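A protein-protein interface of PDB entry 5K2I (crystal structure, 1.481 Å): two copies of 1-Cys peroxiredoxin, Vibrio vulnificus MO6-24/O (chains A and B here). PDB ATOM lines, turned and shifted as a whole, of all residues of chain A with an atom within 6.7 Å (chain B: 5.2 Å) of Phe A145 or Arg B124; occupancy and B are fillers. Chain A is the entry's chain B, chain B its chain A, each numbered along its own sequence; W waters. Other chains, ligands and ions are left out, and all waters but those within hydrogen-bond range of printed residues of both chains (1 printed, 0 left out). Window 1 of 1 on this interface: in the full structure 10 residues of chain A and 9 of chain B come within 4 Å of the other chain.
CB of Ser A49 touches CB of Pro B46, at 3.5 Å. Phe B117 touches Ser A144 (CD1 to O, 3.8 Å). CZ of Phe A145 touches CB of Thr B45, 3.7 Å away. CE1 of Phe A145 touches O of Pro B46 (3.5 Å). Phe A145 touches Phe B117 (CD2 to CZ, 3.5 Å). CE1 of Phe A145 touches NH2 of Arg B124 (3.7 Å).
Of the printed residues of chain B, Ser A49 touches Pro B46 (3.5 Å). Of the printed residues of chain A, Thr B45 touches Phe A145. Printed residues of chain A within 4 Å of Arg B124: Phe A145. The nearest residue of chain A that does not touch Arg B124 is Pro A142 (5.7 Å).
No position is printed for both chains.
Water W1 bridges O of Pro A142 (2.9 Å) and NH1 of Arg B124 (3.3 Å).
Hydrophobic or aromatic side chains of chain A that line the printed part of chain B: Phe A145.
The backbone carbonyl oxygen (O) of Pro B46 lies within hydrogen-bond range of the guanidinium group (NH2) of Arg B124 (3.2 Å). The side-chain hydroxyl (OG1) of Thr B47 lies within hydrogen-bond range of the guanidinium group (NE) of Arg B124 (2.8 Å). NH1 of Arg B124 is in salt-bridge range of OE1 of Glu B140 (2.9 Å).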
ATOM      1  N   SER A  49      12.764  11.801   1.819  1.00  0.00           N
ATOM      2  CA  SER A  49      13.738  10.776   2.186  1.00  0.00           C
ATOM      3  C   SER A  49      13.066   9.502   2.689  1.00  0.00           C
ATOM      4  O   SER A  49      13.716   8.461   2.808  1.00  0.00           O
ATOM      5  CB  SER A  49      14.703  11.303   3.249  1.00  0.00           C
ATOM      6  OG  SER A  49      14.018  11.700   4.425  1.00  0.00           O
ATOM      7  N   ALA A 141      10.393   5.517  11.625  1.00  0.00           N
ATOM      8  CA  ALA A 141      10.599   6.421  12.749  1.00  0.00           C
ATOM      9  C   ALA A 141      11.346   7.632  12.215  1.00  0.00           C
ATOM     10  O   ALA A 141      12.576   7.693  12.282  1.00  0.00           O
ATOM     11  CB  ALA A 141      11.366   5.741  13.862  1.00  0.00           C
ATOM     12  N   PRO A 142      10.602   8.588  11.646  1.00  0.00           N
ATOM     13  CA  PRO A 142      11.165   9.733  10.926  1.00  0.00           C
ATOM     14  C   PRO A 142      12.106  10.596  11.773  1.00  0.00           C
ATOM     15  O   PRO A 142      13.059  11.150  11.228  1.00  0.00           O
ATOM     16  CB  PRO A 142       9.918  10.530  10.504  1.00  0.00           C
ATOM     17  CG  PRO A 142       8.794   9.998  11.352  1.00  0.00           C
ATOM     18  CD  PRO A 142       9.129   8.570  11.592  1.00  0.00           C
ATOM     19  N   LYS A 143      11.841  10.704  13.072  1.00  0.00           N
ATOM     20  CA  LYS A 143      12.673  11.534  13.946  1.00  0.00           C
ATOM     21  C   LYS A 143      14.098  10.988  14.017  1.00  0.00           C
ATOM     22  O   LYS A 143      15.052  11.742  14.250  1.00  0.00           O
ATOM     23  CB  LYS A 143      12.062  11.621  15.344  1.00  0.00           C
ATOM     24  CG  LYS A 143      10.775  12.418  15.391  1.00  0.00           C
ATOM     25  CD  LYS A 143      10.145  12.371  16.774  1.00  0.00           C
ATOM     26  CE  LYS A 143       8.817  13.113  16.791  1.00  0.00           C
ATOM     27  NZ  LYS A 143       8.151  13.016  18.117  1.00  0.00           N
ATOM     28  N   SER A 144      14.239   9.682  13.797  1.00  0.00           N
ATOM     29  CA  SER A 144      15.550   9.035  13.848  1.00  0.00           C
ATOM     30  C   SER A 144      16.038   8.581  12.468  1.00  0.00           C
ATOM     31  O   SER A 144      17.013   7.837  12.351  1.00  0.00           O
ATOM     32  CB  SER A 144      15.504   7.853  14.805  1.00  0.00           C
ATOM     33  OG  SER A 144      15.055   8.279  16.082  1.00  0.00           O
ATOM     34  N   PHE A 145      15.351   9.047  11.427  1.00  0.00           N
ATOM     35  CA  PHE A 145      15.709   8.787  10.036  1.00  0.00           C
ATOM     36  C   PHE A 145      15.777   7.296   9.713  1.00  0.00           C
ATOM     37  O   PHE A 145      16.568   6.868   8.880  1.00  0.00           O
ATOM     38  CB  PHE A 145      17.029   9.493   9.692  1.00  0.00           C
ATOM     39  CG  PHE A 145      16.932  10.987   9.775  1.00  0.00           C
ATOM     40  CD1 PHE A 145      16.469  11.718   8.702  1.00  0.00           C
ATOM     41  CD2 PHE A 145      17.267  11.657  10.940  1.00  0.00           C
ATOM     42  CE1 PHE A 145      16.359  13.094   8.777  1.00  0.00           C
ATOM     43  CE2 PHE A 145      17.161  13.037  11.021  1.00  0.00           C
ATOM     44  CZ  PHE A 145      16.715  13.753   9.938  1.00  0.00           C
ATOM     45  N   GLU A 146      14.907   6.525  10.360  1.00  0.00           N
ATOM     46  CA  GLU A 146      14.770   5.108  10.047  1.00  0.00           C
ATOM     47  C   GLU A 146      13.645   4.926   9.046  1.00  0.00           C
ATOM     48  O   GLU A 146      12.520   5.370   9.290  1.00  0.00           O
ATOM     49  CB  GLU A 146      14.509   4.299  11.306  1.00  0.00           C
ATOM     50  CG  GLU A 146      15.685   4.282  12.268  1.00  0.00           C
ATOM     51  CD  GLU A 146      15.372   3.518  13.533  1.00  0.00           C
ATOM     52  OE1 GLU A 146      14.433   3.925  14.250  1.00  0.00           O
ATOM     53  OE2 GLU A 146      16.052   2.507  13.803  1.00  0.00           O
ATOM     54  N   VAL A 147      13.958   4.293   7.920  1.00  0.00           N
ATOM     55  CA  VAL A 147      13.008   4.154   6.819  1.00  0.00           C
ATOM     56  C   VAL A 147      12.704   2.692   6.493  1.00  0.00           C
ATOM     57  O   VAL A 147      13.549   1.804   6.668  1.00  0.00           O
ATOM     58  CB  VAL A 147      13.526   4.858   5.554  1.00  0.00           C
ATOM     59  CG1 VAL A 147      13.735   6.338   5.835  1.00  0.00           C
ATOM     60  CG2 VAL A 147      14.824   4.209   5.067  1.00  0.00           C
ATOM     61  N   ALA B  39      15.762  26.149  10.224  1.00  0.00           N
ATOM     62  CA  ALA B  39      16.401  25.100  11.002  1.00  0.00           C
ATOM     63  C   ALA B  39      16.152  23.721  10.423  1.00  0.00           C
ATOM     64  O   ALA B  39      15.116  23.474   9.789  1.00  0.00           O
ATOM     65  CB  ALA B  39      15.903  25.143  12.444  1.00  0.00           C
ATOM     66  N   VAL B  40      17.102  22.829  10.689  1.00  0.00           N
ATOM     67  CA  VAL B  40      17.027  21.425  10.309  1.00  0.00           C
ATOM     68  C   VAL B  40      17.416  20.578  11.509  1.00  0.00           C
ATOM     69  O   VAL B  40      18.004  21.091  12.462  1.00  0.00           O
ATOM     70  CB  VAL B  40      17.959  21.100   9.115  1.00  0.00           C
ATOM     71  CG1 VAL B  40      17.493  21.844   7.867  1.00  0.00           C
ATOM     72  CG2 VAL B  40      19.430  21.416   9.461  1.00  0.00           C
ATOM     73  N   PRO B  41      17.083  19.277  11.477  1.00  0.00           N
ATOM     74  CA  PRO B  41      17.473  18.413  12.590  1.00  0.00           C
ATOM     75  C   PRO B  41      18.957  18.109  12.604  1.00  0.00           C
ATOM     76  O   PRO B  41      19.494  17.692  13.638  1.00  0.00           O
ATOM     77  CB  PRO B  41      16.680  17.126  12.341  1.00  0.00           C
ATOM     78  CG  PRO B  41      15.566  17.527  11.414  1.00  0.00           C
ATOM     79  CD  PRO B  41      16.169  18.589  10.545  1.00  0.00           C
ATOM     80  N   THR B  45      21.727  15.939   7.005  1.00  0.00           N
ATOM     81  CA  THR B  45      20.574  15.036   7.082  1.00  0.00           C
ATOM     82  C   THR B  45      19.580  15.344   5.962  1.00  0.00           C
ATOM     83  O   THR B  45      19.560  16.446   5.411  1.00  0.00           O
ATOM     84  CB  THR B  45      19.840  15.094   8.465  1.00  0.00           C
ATOM     85  OG1 THR B  45      19.172  16.353   8.626  1.00  0.00           O
ATOM     86  CG2 THR B  45      20.808  14.835   9.600  1.00  0.00           C
ATOM     87  N   PRO B  46      18.748  14.361   5.605  1.00  0.00           N
ATOM     88  CA  PRO B  46      17.838  14.645   4.496  1.00  0.00           C
ATOM     89  C   PRO B  46      16.610  15.420   4.953  1.00  0.00           C
ATOM     90  O   PRO B  46      16.019  15.141   6.005  1.00  0.00           O
ATOM     91  CB  PRO B  46      17.478  13.255   3.971  1.00  0.00           C
ATOM     92  CG  PRO B  46      17.714  12.333   5.108  1.00  0.00           C
ATOM     93  CD  PRO B  46      18.779  12.938   5.981  1.00  0.00           C
ATOM     94  N   THR B  47      16.283  16.445   4.174  1.00  0.00           N
ATOM     95  CA  THR B  47      15.076  17.248   4.326  1.00  0.00           C
ATOM     96  C   THR B  47      14.642  17.530   2.899  1.00  0.00           C
ATOM     97  O   THR B  47      15.505  17.644   2.026  1.00  0.00           O
ATOM     98  CB  THR B  47      15.335  18.567   5.099  1.00  0.00           C
ATOM     99  OG1 THR B  47      15.674  18.275   6.463  1.00  0.00           O
ATOM    100  CG2 THR B  47      14.118  19.488   5.061  1.00  0.00           C
ATOM    101  N   PHE B 117      19.664   8.380  17.181  1.00  0.00           N
ATOM    102  CA  PHE B 117      20.188   8.967  15.957  1.00  0.00           C
ATOM    103  C   PHE B 117      21.175  10.086  16.277  1.00  0.00           C
ATOM    104  O   PHE B 117      22.302  10.095  15.781  1.00  0.00           O
ATOM    105  CB  PHE B 117      19.072   9.522  15.065  1.00  0.00           C
ATOM    106  CG  PHE B 117      19.589  10.382  13.952  1.00  0.00           C
ATOM    107  CD1 PHE B 117      20.173   9.810  12.837  1.00  0.00           C
ATOM    108  CD2 PHE B 117      19.540  11.770  14.049  1.00  0.00           C
ATOM    109  CE1 PHE B 117      20.684  10.597  11.819  1.00  0.00           C
ATOM    110  CE2 PHE B 117      20.059  12.572  13.040  1.00  0.00           C
ATOM    111  CZ  PHE B 117      20.631  11.985  11.924  1.00  0.00           C
ATOM    112  N   SER B 122      16.955  20.008  16.633  1.00  0.00           N
ATOM    113  CA  SER B 122      15.906  20.975  16.350  1.00  0.00           C
ATOM    114  C   SER B 122      14.827  20.382  15.462  1.00  0.00           C
ATOM    115  O   SER B 122      15.113  19.569  14.581  1.00  0.00           O
ATOM    116  CB  SER B 122      16.485  22.204  15.650  1.00  0.00           C
ATOM    117  OG  SER B 122      15.486  23.189  15.442  1.00  0.00           O
ATOM    118  N   GLN B 123      13.591  20.809  15.681  1.00  0.00           N
ATOM    119  CA  GLN B 123      12.533  20.630  14.688  1.00  0.00           C
ATOM    120  C   GLN B 123      12.866  21.461  13.457  1.00  0.00           C
ATOM    121  O   GLN B 123      13.644  22.424  13.546  1.00  0.00           O
ATOM    122  CB  GLN B 123      11.179  21.049  15.260  1.00  0.00           C
ATOM    123  CG  GLN B 123      10.714  20.166  16.418  1.00  0.00           C
ATOM    124  CD  GLN B 123       9.470  20.724  17.102  1.00  0.00           C
ATOM    125  OE1 GLN B 123       9.431  20.871  18.333  1.00  0.00           O
ATOM    126  NE2 GLN B 123       8.459  21.041  16.313  1.00  0.00           N
ATOM    127  N   ARG B 124      12.234  21.125  12.337  1.00  0.00           N
ATOM    128  CA  ARG B 124      12.298  21.955  11.137  1.00  0.00           C
ATOM    129  C   ARG B 124      11.358  23.140  11.263  1.00  0.00           C
ATOM    130  O   ARG B 124      10.183  22.967  11.559  1.00  0.00           O
ATOM    131  CB  ARG B 124      11.920  21.140   9.899  1.00  0.00           C
ATOM    132  CG  ARG B 124      12.892  20.026   9.596  1.00  0.00           C
ATOM    133  CD  ARG B 124      12.529  19.295   8.304  1.00  0.00           C
ATOM    134  NE  ARG B 124      13.418  18.158   8.082  1.00  0.00           N
ATOM    135  CZ  ARG B 124      13.206  16.949   8.590  1.00  0.00           C
ATOM    136  NH1 ARG B 124      12.136  16.723   9.342  1.00  0.00           N
ATOM    137  NH2 ARG B 124      14.065  15.964   8.358  1.00  0.00           N
ATOM    138  N   TYR B 125      11.880  24.345  11.051  1.00  0.00           N
ATOM    139  CA  TYR B 125      11.056  25.534  11.038  1.00  0.00           C
ATOM    140  C   TYR B 125      11.737  26.617  10.214  1.00  0.00           C
ATOM    141  O   TYR B 125      12.938  26.531   9.915  1.00  0.00           O
ATOM    142  CB  TYR B 125      10.776  26.043  12.475  1.00  0.00           C
ATOM    143  CG  TYR B 125      12.018  26.526  13.221  1.00  0.00           C
ATOM    144  CD1 TYR B 125      12.559  27.783  12.973  1.00  0.00           C
ATOM    145  CD2 TYR B 125      12.661  25.712  14.148  1.00  0.00           C
ATOM    146  CE1 TYR B 125      13.700  28.217  13.627  1.00  0.00           C
ATOM    147  CE2 TYR B 125      13.799  26.146  14.821  1.00  0.00           C
ATOM    148  CZ  TYR B 125      14.315  27.394  14.542  1.00  0.00           C
ATOM    149  OH  TYR B 125      15.456  27.810  15.193  1.00  0.00           O
ATOM    150  N   ALA B 126      10.987  27.657   9.889  1.00  0.00           N
ATOM    151  CA  ALA B 126      11.568  28.830   9.258  1.00  0.00           C
ATOM    152  C   ALA B 126      10.896  30.065   9.809  1.00  0.00           C
ATOM    153  O   ALA B 126       9.698  30.051  10.128  1.00  0.00           O
ATOM    154  CB  ALA B 126      11.431  28.766   7.742  1.00  0.00           C
ATOM    155  N   ASN B 138       6.986  29.447  10.809  1.00  0.00           N
ATOM    156  CA  ASN B 138       6.342  28.274  10.220  1.00  0.00           C
ATOM    157  C   ASN B 138       7.058  27.033  10.715  1.00  0.00           C
ATOM    158  O   ASN B 138       8.253  26.881  10.479  1.00  0.00           O
ATOM    159  CB  ASN B 138       6.382  28.318   8.684  1.00  0.00           C
ATOM    160  CG  ASN B 138       5.634  29.502   8.102  1.00  0.00           C
ATOM    161  OD1 ASN B 138       4.669  29.982   8.683  1.00  0.00           O
ATOM    162  ND2 ASN B 138       6.077  29.971   6.934  1.00  0.00           N
ATOM    163  N   VAL B 139       6.341  26.154  11.407  1.00  0.00           N
ATOM    164  CA  VAL B 139       6.927  24.946  11.983  1.00  0.00           C
ATOM    165  C   VAL B 139       6.390  23.717  11.252  1.00  0.00           C
ATOM    166  O   VAL B 139       5.187  23.632  10.965  1.00  0.00           O
ATOM    167  CB  VAL B 139       6.620  24.848  13.501  1.00  0.00           C
ATOM    168  CG1 VAL B 139       7.273  23.622  14.095  1.00  0.00           C
ATOM    169  CG2 VAL B 139       7.100  26.114  14.224  1.00  0.00           C
ATOM    170  N   GLU B 140       7.275  22.778  10.933  1.00  0.00           N
ATOM    171  CA  GLU B 140       6.840  21.533  10.288  1.00  0.00           C
ATOM    172  C   GLU B 140       5.819  20.799  11.160  1.00  0.00           C
ATOM    173  O   GLU B 140       5.962  20.727  12.377  1.00  0.00           O
ATOM    174  CB  GLU B 140       8.046  20.621   9.998  1.00  0.00           C
ATOM    175  CG  GLU B 140       7.696  19.348   9.209  1.00  0.00           C
ATOM    176  CD  GLU B 140       8.841  18.353   9.073  1.00  0.00           C
ATOM    177  OE1 GLU B 140       9.759  18.334   9.923  1.00  0.00           O
ATOM    178  OE2 GLU B 140       8.799  17.554   8.110  1.00  0.00           O
HETATM  179  O   HOH W   1      13.219  14.068  11.018  1.00  0.00           O
